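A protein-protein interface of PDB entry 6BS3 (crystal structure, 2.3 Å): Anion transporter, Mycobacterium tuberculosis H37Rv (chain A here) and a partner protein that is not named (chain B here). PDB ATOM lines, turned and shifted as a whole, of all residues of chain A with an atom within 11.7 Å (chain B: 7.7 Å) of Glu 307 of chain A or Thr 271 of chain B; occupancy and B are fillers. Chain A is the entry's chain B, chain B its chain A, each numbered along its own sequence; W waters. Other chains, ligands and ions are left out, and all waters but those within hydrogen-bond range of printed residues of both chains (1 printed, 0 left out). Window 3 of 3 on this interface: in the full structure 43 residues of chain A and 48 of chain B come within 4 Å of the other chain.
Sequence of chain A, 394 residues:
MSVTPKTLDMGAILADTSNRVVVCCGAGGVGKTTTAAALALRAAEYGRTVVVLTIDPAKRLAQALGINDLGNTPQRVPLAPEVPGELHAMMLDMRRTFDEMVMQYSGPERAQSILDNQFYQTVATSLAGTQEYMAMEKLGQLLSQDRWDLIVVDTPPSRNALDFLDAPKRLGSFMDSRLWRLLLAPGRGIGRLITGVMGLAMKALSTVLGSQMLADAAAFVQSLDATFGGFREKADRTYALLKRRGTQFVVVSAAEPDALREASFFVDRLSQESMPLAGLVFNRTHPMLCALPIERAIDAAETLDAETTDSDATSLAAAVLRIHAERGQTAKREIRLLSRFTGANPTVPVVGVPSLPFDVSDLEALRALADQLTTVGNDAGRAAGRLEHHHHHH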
ATOM      1  N   ARG A 296      11.941  24.031  13.651  1.00  0.00           N
ATOM      2  CA  ARG A 296      11.843  24.044  15.113  1.00  0.00           C
ATOM      3  C   ARG A 296      11.150  25.300  15.631  1.00  0.00           C
ATOM      4  O   ARG A 296      10.366  25.204  16.571  1.00  0.00           O
ATOM      5  CB  ARG A 296      13.236  23.926  15.752  1.00  0.00           C
ATOM      6  CG  ARG A 296      13.678  22.489  15.998  1.00  0.00           C
ATOM      7  CD  ARG A 296      13.749  22.163  17.482  1.00  0.00           C
ATOM      8  NE  ARG A 296      14.979  22.665  18.101  1.00  0.00           N
ATOM      9  CZ  ARG A 296      15.211  22.673  19.411  1.00  0.00           C
ATOM     10  NH1 ARG A 296      14.295  22.219  20.259  1.00  0.00           N
ATOM     11  NH2 ARG A 296      16.357  23.145  19.883  1.00  0.00           N
ATOM     12  N   ALA A 297      11.450  26.471  15.029  1.00  0.00           N
ATOM     13  CA  ALA A 297      10.879  27.768  15.413  1.00  0.00           C
ATOM     14  C   ALA A 297       9.369  27.848  15.158  1.00  0.00           C
ATOM     15  O   ALA A 297       8.639  28.349  16.019  1.00  0.00           O
ATOM     16  CB  ALA A 297      11.605  28.899  14.695  1.00  0.00           C
ATOM     17  N   ILE A 298       8.905  27.346  13.991  1.00  0.00           N
ATOM     18  CA  ILE A 298       7.487  27.327  13.624  1.00  0.00           C
ATOM     19  C   ILE A 298       6.730  26.393  14.580  1.00  0.00           C
ATOM     20  O   ILE A 298       5.700  26.795  15.125  1.00  0.00           O
ATOM     21  CB  ILE A 298       7.262  26.966  12.124  1.00  0.00           C
ATOM     22  CG1 ILE A 298       7.988  27.961  11.186  1.00  0.00           C
ATOM     23  CG2 ILE A 298       5.758  26.898  11.785  1.00  0.00           C
ATOM     24  CD1 ILE A 298       8.399  27.375   9.836  1.00  0.00           C
ATOM     25  N   ASP A 299       7.268  25.170  14.808  1.00  0.00           N
ATOM     26  CA  ASP A 299       6.693  24.165  15.704  1.00  0.00           C
ATOM     27  C   ASP A 299       6.619  24.655  17.152  1.00  0.00           C
ATOM     28  O   ASP A 299       5.604  24.424  17.807  1.00  0.00           O
ATOM     29  CB  ASP A 299       7.455  22.829  15.606  1.00  0.00           C
ATOM     30  CG  ASP A 299       7.156  21.997  14.366  1.00  0.00           C
ATOM     31  OD1 ASP A 299       6.127  22.269  13.692  1.00  0.00           O
ATOM     32  OD2 ASP A 299       7.939  21.067  14.073  1.00  0.00           O
ATOM     33  N   ALA A 300       7.666  25.362  17.633  1.00  0.00           N
ATOM     34  CA  ALA A 300       7.705  25.936  18.984  1.00  0.00           C
ATOM     35  C   ALA A 300       6.626  27.016  19.139  1.00  0.00           C
ATOM     36  O   ALA A 300       6.008  27.111  20.198  1.00  0.00           O
ATOM     37  CB  ALA A 300       9.078  26.519  19.276  1.00  0.00           C
ATOM     38  N   ALA A 301       6.383  27.802  18.067  1.00  0.00           N
ATOM     39  CA  ALA A 301       5.363  28.851  18.027  1.00  0.00           C
ATOM     40  C   ALA A 301       3.960  28.241  17.921  1.00  0.00           C
ATOM     41  O   ALA A 301       3.022  28.783  18.506  1.00  0.00           O
ATOM     42  CB  ALA A 301       5.620  29.787  16.854  1.00  0.00           C
ATOM     43  N   GLU A 302       3.826  27.118  17.181  1.00  0.00           N
ATOM     44  CA  GLU A 302       2.563  26.399  16.977  1.00  0.00           C
ATOM     45  C   GLU A 302       2.053  25.700  18.250  1.00  0.00           C
ATOM     46  O   GLU A 302       0.836  25.617  18.444  1.00  0.00           O
ATOM     47  CB  GLU A 302       2.657  25.426  15.791  1.00  0.00           C
ATOM     48  CG  GLU A 302       2.486  26.106  14.440  1.00  0.00           C
ATOM     49  CD  GLU A 302       2.617  25.223  13.211  1.00  0.00           C
ATOM     50  OE1 GLU A 302       3.406  24.251  13.243  1.00  0.00           O
ATOM     51  OE2 GLU A 302       1.935  25.519  12.204  1.00  0.00           O
ATOM     52  N   THR A 303       2.979  25.217  19.118  1.00  0.00           N
ATOM     53  CA  THR A 303       2.627  24.584  20.397  1.00  0.00           C
ATOM     54  C   THR A 303       2.079  25.653  21.352  1.00  0.00           C
ATOM     55  O   THR A 303       1.131  25.385  22.092  1.00  0.00           O
ATOM     56  CB  THR A 303       3.798  23.774  21.007  1.00  0.00           C
ATOM     57  OG1 THR A 303       4.926  24.617  21.240  1.00  0.00           O
ATOM     58  CG2 THR A 303       4.198  22.565  20.166  1.00  0.00           C
ATOM     59  N   LEU A 304       2.646  26.875  21.288  1.00  0.00           N
ATOM     60  CA  LEU A 304       2.231  28.027  22.091  1.00  0.00           C
ATOM     61  C   LEU A 304       0.869  28.571  21.648  1.00  0.00           C
ATOM     62  O   LEU A 304       0.139  29.113  22.480  1.00  0.00           O
ATOM     63  CB  LEU A 304       3.296  29.138  22.049  1.00  0.00           C
ATOM     64  CG  LEU A 304       4.619  28.860  22.786  1.00  0.00           C
ATOM     65  CD1 LEU A 304       5.710  29.799  22.312  1.00  0.00           C
ATOM     66  CD2 LEU A 304       4.454  28.969  24.300  1.00  0.00           C
ATOM     67  N   ASP A 305       0.528  28.416  20.345  1.00  0.00           N
ATOM     68  CA  ASP A 305      -0.744  28.845  19.748  1.00  0.00           C
ATOM     69  C   ASP A 305      -1.922  28.042  20.304  1.00  0.00           C
ATOM     70  O   ASP A 305      -2.982  28.616  20.557  1.00  0.00           O
ATOM     71  CB  ASP A 305      -0.712  28.709  18.212  1.00  0.00           C
ATOM     72  CG  ASP A 305       0.123  29.734  17.468  1.00  0.00           C
ATOM     73  OD1 ASP A 305       0.031  30.935  17.804  1.00  0.00           O
ATOM     74  OD2 ASP A 305       0.840  29.342  16.525  1.00  0.00           O
ATOM     75  N   ALA A 306      -1.738  26.717  20.480  1.00  0.00           N
ATOM     76  CA  ALA A 306      -2.761  25.810  21.006  1.00  0.00           C
ATOM     77  C   ALA A 306      -2.987  26.014  22.508  1.00  0.00           C
ATOM     78  O   ALA A 306      -4.129  25.921  22.968  1.00  0.00           O
ATOM     79  CB  ALA A 306      -2.375  24.365  20.725  1.00  0.00           C
ATOM     80  N   GLU A 307      -1.899  26.289  23.266  1.00  0.00           N
ATOM     81  CA  GLU A 307      -1.926  26.511  24.714  1.00  0.00           C
ATOM     82  C   GLU A 307      -2.581  27.857  25.072  1.00  0.00           C
ATOM     83  O   GLU A 307      -1.917  28.811  25.482  1.00  0.00           O
ATOM     84  CB  GLU A 307      -0.517  26.375  25.320  1.00  0.00           C
ATOM     85  CG  GLU A 307       0.020  24.953  25.324  1.00  0.00           C
ATOM     86  CD  GLU A 307       0.802  24.552  26.562  1.00  0.00           C
ATOM     87  OE1 GLU A 307       1.406  25.439  27.208  1.00  0.00           O
ATOM     88  OE2 GLU A 307       0.812  23.342  26.886  1.00  0.00           O
ATOM     89  N   THR A 314       0.981  33.545  26.752  1.00  0.00           N
ATOM     90  CA  THR A 314       1.878  34.678  26.541  1.00  0.00           C
ATOM     91  C   THR A 314       2.221  34.809  25.027  1.00  0.00           C
ATOM     92  O   THR A 314       3.089  34.104  24.492  1.00  0.00           O
ATOM     93  CB  THR A 314       3.095  34.639  27.513  1.00  0.00           C
ATOM     94  OG1 THR A 314       3.915  35.791  27.308  1.00  0.00           O
ATOM     95  CG2 THR A 314       3.932  33.350  27.416  1.00  0.00           C
ATOM     96  N   SER A 315       1.502  35.726  24.352  1.00  0.00           N
ATOM     97  CA  SER A 315       1.610  36.003  22.917  1.00  0.00           C
ATOM     98  C   SER A 315       2.983  36.549  22.464  1.00  0.00           C
ATOM     99  O   SER A 315       3.287  36.497  21.269  1.00  0.00           O
ATOM    100  CB  SER A 315       0.482  36.931  22.467  1.00  0.00           C
ATOM    101  OG  SER A 315       0.291  38.027  23.349  1.00  0.00           O
ATOM    102  N   LEU A 316       3.807  37.049  23.412  1.00  0.00           N
ATOM    103  CA  LEU A 316       5.135  37.606  23.147  1.00  0.00           C
ATOM    104  C   LEU A 316       6.110  36.560  22.604  1.00  0.00           C
ATOM    105  O   LEU A 316       6.687  36.779  21.541  1.00  0.00           O
ATOM    106  CB  LEU A 316       5.702  38.300  24.407  1.00  0.00           C
ATOM    107  CG  LEU A 316       7.059  39.019  24.286  1.00  0.00           C
ATOM    108  CD1 LEU A 316       6.950  40.294  23.454  1.00  0.00           C
ATOM    109  CD2 LEU A 316       7.603  39.368  25.651  1.00  0.00           C
ATOM    110  N   ALA A 317       6.273  35.427  23.319  1.00  0.00           N
ATOM    111  CA  ALA A 317       7.180  34.333  22.951  1.00  0.00           C
ATOM    112  C   ALA A 317       6.922  33.757  21.555  1.00  0.00           C
ATOM    113  O   ALA A 317       7.871  33.610  20.784  1.00  0.00           O
ATOM    114  CB  ALA A 317       7.133  33.229  24.000  1.00  0.00           C
ATOM    115  N   ALA A 318       5.647  33.462  21.220  1.00  0.00           N
ATOM    116  CA  ALA A 318       5.274  32.909  19.916  1.00  0.00           C
ATOM    117  C   ALA A 318       5.527  33.893  18.769  1.00  0.00           C
ATOM    118  O   ALA A 318       5.954  33.462  17.696  1.00  0.00           O
ATOM    119  CB  ALA A 318       3.822  32.464  19.923  1.00  0.00           C
ATOM    120  N   ALA A 319       5.283  35.204  18.997  1.00  0.00           N
ATOM    121  CA  ALA A 319       5.503  36.249  17.995  1.00  0.00           C
ATOM    122  C   ALA A 319       6.998  36.386  17.705  1.00  0.00           C
ATOM    123  O   ALA A 319       7.377  36.486  16.538  1.00  0.00           O
ATOM    124  CB  ALA A 319       4.922  37.574  18.466  1.00  0.00           C
ATOM    125  N   LEU A 321       9.228  34.033  17.964  1.00  0.00           N
ATOM    126  CA  LEU A 321       9.557  32.830  17.195  1.00  0.00           C
ATOM    127  C   LEU A 321       9.146  33.019  15.731  1.00  0.00           C
ATOM    128  O   LEU A 321       9.837  32.539  14.829  1.00  0.00           O
ATOM    129  CB  LEU A 321       8.828  31.597  17.783  1.00  0.00           C
ATOM    130  CG  LEU A 321       9.173  31.099  19.206  1.00  0.00           C
ATOM    131  CD1 LEU A 321       8.266  29.977  19.675  1.00  0.00           C
ATOM    132  CD2 LEU A 321      10.629  30.722  19.335  1.00  0.00           C
ATOM    133  N   ARG A 322       8.014  33.714  15.507  1.00  0.00           N
ATOM    134  CA  ARG A 322       7.489  34.011  14.173  1.00  0.00           C
ATOM    135  C   ARG A 322       8.346  35.051  13.430  1.00  0.00           C
ATOM    136  O   ARG A 322       8.399  35.006  12.206  1.00  0.00           O
ATOM    137  CB  ARG A 322       6.008  34.426  14.227  1.00  0.00           C
ATOM    138  CG  ARG A 322       5.061  33.277  14.539  1.00  0.00           C
ATOM    139  CD  ARG A 322       3.835  33.283  13.644  1.00  0.00           C
ATOM    140  NE  ARG A 322       2.862  32.268  14.056  1.00  0.00           N
ATOM    141  CZ  ARG A 322       2.837  31.016  13.607  1.00  0.00           C
ATOM    142  NH1 ARG A 322       3.730  30.605  12.715  1.00  0.00           N
ATOM    143  NH2 ARG A 322       1.918  30.166  14.045  1.00  0.00           N
ATOM    144  N   SER B 264      10.009  36.883  30.150  1.00  0.00           N
ATOM    145  CA  SER B 264       8.772  36.390  29.530  1.00  0.00           C
ATOM    146  C   SER B 264       9.075  35.519  28.295  1.00  0.00           C
ATOM    147  O   SER B 264       8.415  34.492  28.101  1.00  0.00           O
ATOM    148  CB  SER B 264       7.856  37.553  29.149  1.00  0.00           C
ATOM    149  OG  SER B 264       6.614  37.111  28.627  1.00  0.00           O
ATOM    150  N   VAL B 265      10.087  35.925  27.481  1.00  0.00           N
ATOM    151  CA  VAL B 265      10.538  35.214  26.272  1.00  0.00           C
ATOM    152  C   VAL B 265      11.158  33.854  26.655  1.00  0.00           C
ATOM    153  O   VAL B 265      10.775  32.838  26.073  1.00  0.00           O
ATOM    154  CB  VAL B 265      11.478  36.074  25.371  1.00  0.00           C
ATOM    155  CG1 VAL B 265      11.905  35.313  24.118  1.00  0.00           C
ATOM    156  CG2 VAL B 265      10.822  37.394  24.982  1.00  0.00           C
ATOM    157  N   ARG B 266      12.074  33.842  27.655  1.00  0.00           N
ATOM    158  CA  ARG B 266      12.741  32.641  28.180  1.00  0.00           C
ATOM    159  C   ARG B 266      11.727  31.636  28.751  1.00  0.00           C
ATOM    160  O   ARG B 266      11.891  30.429  28.557  1.00  0.00           O
ATOM    161  CB  ARG B 266      13.778  33.017  29.253  1.00  0.00           C
ATOM    162  CG  ARG B 266      15.123  32.319  29.073  1.00  0.00           C
ATOM    163  CD  ARG B 266      16.065  32.534  30.247  1.00  0.00           C
ATOM    164  NE  ARG B 266      16.575  33.906  30.328  1.00  0.00           N
ATOM    165  CZ  ARG B 266      17.678  34.341  29.721  1.00  0.00           C
ATOM    166  NH1 ARG B 266      18.400  33.519  28.968  1.00  0.00           N
ATOM    167  NH2 ARG B 266      18.059  35.605  29.854  1.00  0.00           N
ATOM    168  N   ALA B 267      10.672  32.148  29.430  1.00  0.00           N
ATOM    169  CA  ALA B 267       9.588  31.360  30.023  1.00  0.00           C
ATOM    170  C   ALA B 267       8.741  30.679  28.945  1.00  0.00           C
ATOM    171  O   ALA B 267       8.493  29.477  29.040  1.00  0.00           O
ATOM    172  CB  ALA B 267       8.713  32.242  30.902  1.00  0.00           C
ATOM    173  N   GLY B 268       8.338  31.445  27.930  1.00  0.00           N
ATOM    174  CA  GLY B 268       7.556  30.954  26.800  1.00  0.00           C
ATOM    175  C   GLY B 268       8.317  29.981  25.917  1.00  0.00           C
ATOM    176  O   GLY B 268       7.704  29.169  25.219  1.00  0.00           O
ATOM    177  N   LEU B 269       9.666  30.059  25.943  1.00  0.00           N
ATOM    178  CA  LEU B 269      10.547  29.161  25.197  1.00  0.00           C
ATOM    179  C   LEU B 269      10.632  27.818  25.925  1.00  0.00           C
ATOM    180  O   LEU B 269      10.614  26.778  25.267  1.00  0.00           O
ATOM    181  CB  LEU B 269      11.949  29.771  24.998  1.00  0.00           C
ATOM    182  CG  LEU B 269      12.126  30.741  23.818  1.00  0.00           C
ATOM    183  CD1 LEU B 269      13.274  31.699  24.066  1.00  0.00           C
ATOM    184  CD2 LEU B 269      12.357  30.000  22.512  1.00  0.00           C
ATOM    185  N   LEU B 270      10.695  27.841  27.282  1.00  0.00           N
ATOM    186  CA  LEU B 270      10.733  26.642  28.134  1.00  0.00           C
ATOM    187  C   LEU B 270       9.439  25.828  28.012  1.00  0.00           C
ATOM    188  O   LEU B 270       9.482  24.599  28.070  1.00  0.00           O
ATOM    189  CB  LEU B 270      10.976  27.017  29.607  1.00  0.00           C
ATOM    190  CG  LEU B 270      12.424  27.266  30.035  1.00  0.00           C
ATOM    191  CD1 LEU B 270      12.473  28.017  31.348  1.00  0.00           C
ATOM    192  CD2 LEU B 270      13.199  25.959  30.168  1.00  0.00           C
ATOM    193  N   THR B 271       8.298  26.528  27.842  1.00  0.00           N
ATOM    194  CA  THR B 271       6.949  25.984  27.660  1.00  0.00           C
ATOM    195  C   THR B 271       6.883  25.171  26.358  1.00  0.00           C
ATOM    196  O   THR B 271       6.286  24.095  26.340  1.00  0.00           O
ATOM    197  CB  THR B 271       5.933  27.145  27.691  1.00  0.00           C
ATOM    198  OG1 THR B 271       6.019  27.799  28.957  1.00  0.00           O
ATOM    199  CG2 THR B 271       4.496  26.696  27.441  1.00  0.00           C
ATOM    200  N   ALA B 272       7.518  25.682  25.284  1.00  0.00           N
ATOM    201  CA  ALA B 272       7.570  25.055  23.958  1.00  0.00           C
ATOM    202  C   ALA B 272       8.705  24.016  23.825  1.00  0.00           C
ATOM    203  O   ALA B 272       8.880  23.432  22.750  1.00  0.00           O
ATOM    204  CB  ALA B 272       7.706  26.131  22.890  1.00  0.00           C
ATOM    205  N   GLY B 273       9.439  23.789  24.920  1.00  0.00           N
ATOM    206  CA  GLY B 273      10.557  22.854  24.979  1.00  0.00           C
ATOM    207  C   GLY B 273      11.763  23.326  24.192  1.00  0.00           C
ATOM    208  O   GLY B 273      12.301  22.576  23.371  1.00  0.00           O
ATOM    209  N   VAL B 274      12.165  24.600  24.410  1.00  0.00           N
ATOM    210  CA  VAL B 274      13.302  25.255  23.748  1.00  0.00           C
ATOM    211  C   VAL B 274      14.151  25.990  24.805  1.00  0.00           C
ATOM    212  O   VAL B 274      13.645  26.862  25.516  1.00  0.00           O
ATOM    213  CB  VAL B 274      12.888  26.203  22.568  1.00  0.00           C
ATOM    214  CG1 VAL B 274      14.113  26.763  21.842  1.00  0.00           C
ATOM    215  CG2 VAL B 274      11.957  25.508  21.574  1.00  0.00           C
HETATM  216  O   HOH W   1       6.452  35.360  26.464  1.00  0.00           O
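Arg 296 of chain A touches Gly 273 of chain B (NH1 to O, 3.7 Å). CB of Ala 272 of chain B touches O of Ala 300 of chain A, 3.3 Å away. Ala 300 of chain A touches Val 274 of chain B. Thr 303 of chain A touches Ala 272 of chain B. Leu 304 of chain A touches Thr 271 of chain B. Glu 307 of chain A touches Thr 271 of chain B. Ser 264 of chain B touches Leu 316 of chain A. CG2 of Val 265 of chain B touches CD2 of Leu 316 of chain A (3.8 Å). CA of Gly 268 of chain B touches CB of Ala 317 of chain A, at 3.6 Å. CD2 of Leu 269 of chain B touches CD2 of Leu 321 of chain A, at 3.7 Å.
Water W1 lies within hydrogen-bond range of O of Ser 264 of chain B (2.7 Å), OG1 of Thr 314 of chain A (2.7 Å) and N of Ala 317 of chain A (3.2 Å).
OG1 of Thr 271 of chain B lies within hydrogen-bond range of O of Ala 267 of chain B (3.0 Å). The backbone carbonyl oxygen (O) of Leu 269 of chain B lies within hydrogen-bond range of the backbone NH (N) of Val 274 of chain B (2.8 Å). O of Ala 300 of chain A is in hydrogen-bond range of OG1 of Thr 303 of chain A (2.9 Å).
Printed residues of chain B that touch a printed residue of chain A: Ser 264, Val 265, Gly 268, Leu 269, Thr 271, Ala 272, Gly 273 and Val 274. Hydrophobic or aromatic side chains of chain B within 4 Å of the printed part of chain A: Val 265, Leu 269, Ala 272 and Val 274. Hydrophobic or aromatic side chains of chain A within 4 Å of the printed part of chain B: Ala 300, Leu 304, Leu 316, Ala 317 and Leu 321. Among the printed residues, 12 pairs touch across the chains. Among the printed residues, no Asp or Glu carboxylate lies within 4 Å of a Lys or Arg side-chain nitrogen of the other chain.
OG of Ser 264 of chain B lies within hydrogen-bond range of OG1 of Thr 314 of chain A (3.3 Å).
Glu 307 of chain A touches just one residue of chain B: Thr 271 (3.3 Å). Of chain A, only Leu 304 (3.9 Å) and Glu 307 (3.3 Å) come within 4 Å of Thr 271 of chain B. No residue of chain B comes within 4 Å of Ala 306 of chain A. Of the printed residues of chain A, Leu 269 of chain B touches Leu 321. Printed residues of chain B within 4 Å of Thr 314 of chain A: Ser 264. Of the printed residues of chain A, Val 265 of chain B touches Leu 316 (3.8 Å). Ile 298 of chain A touches none of the printed residues of chain B.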
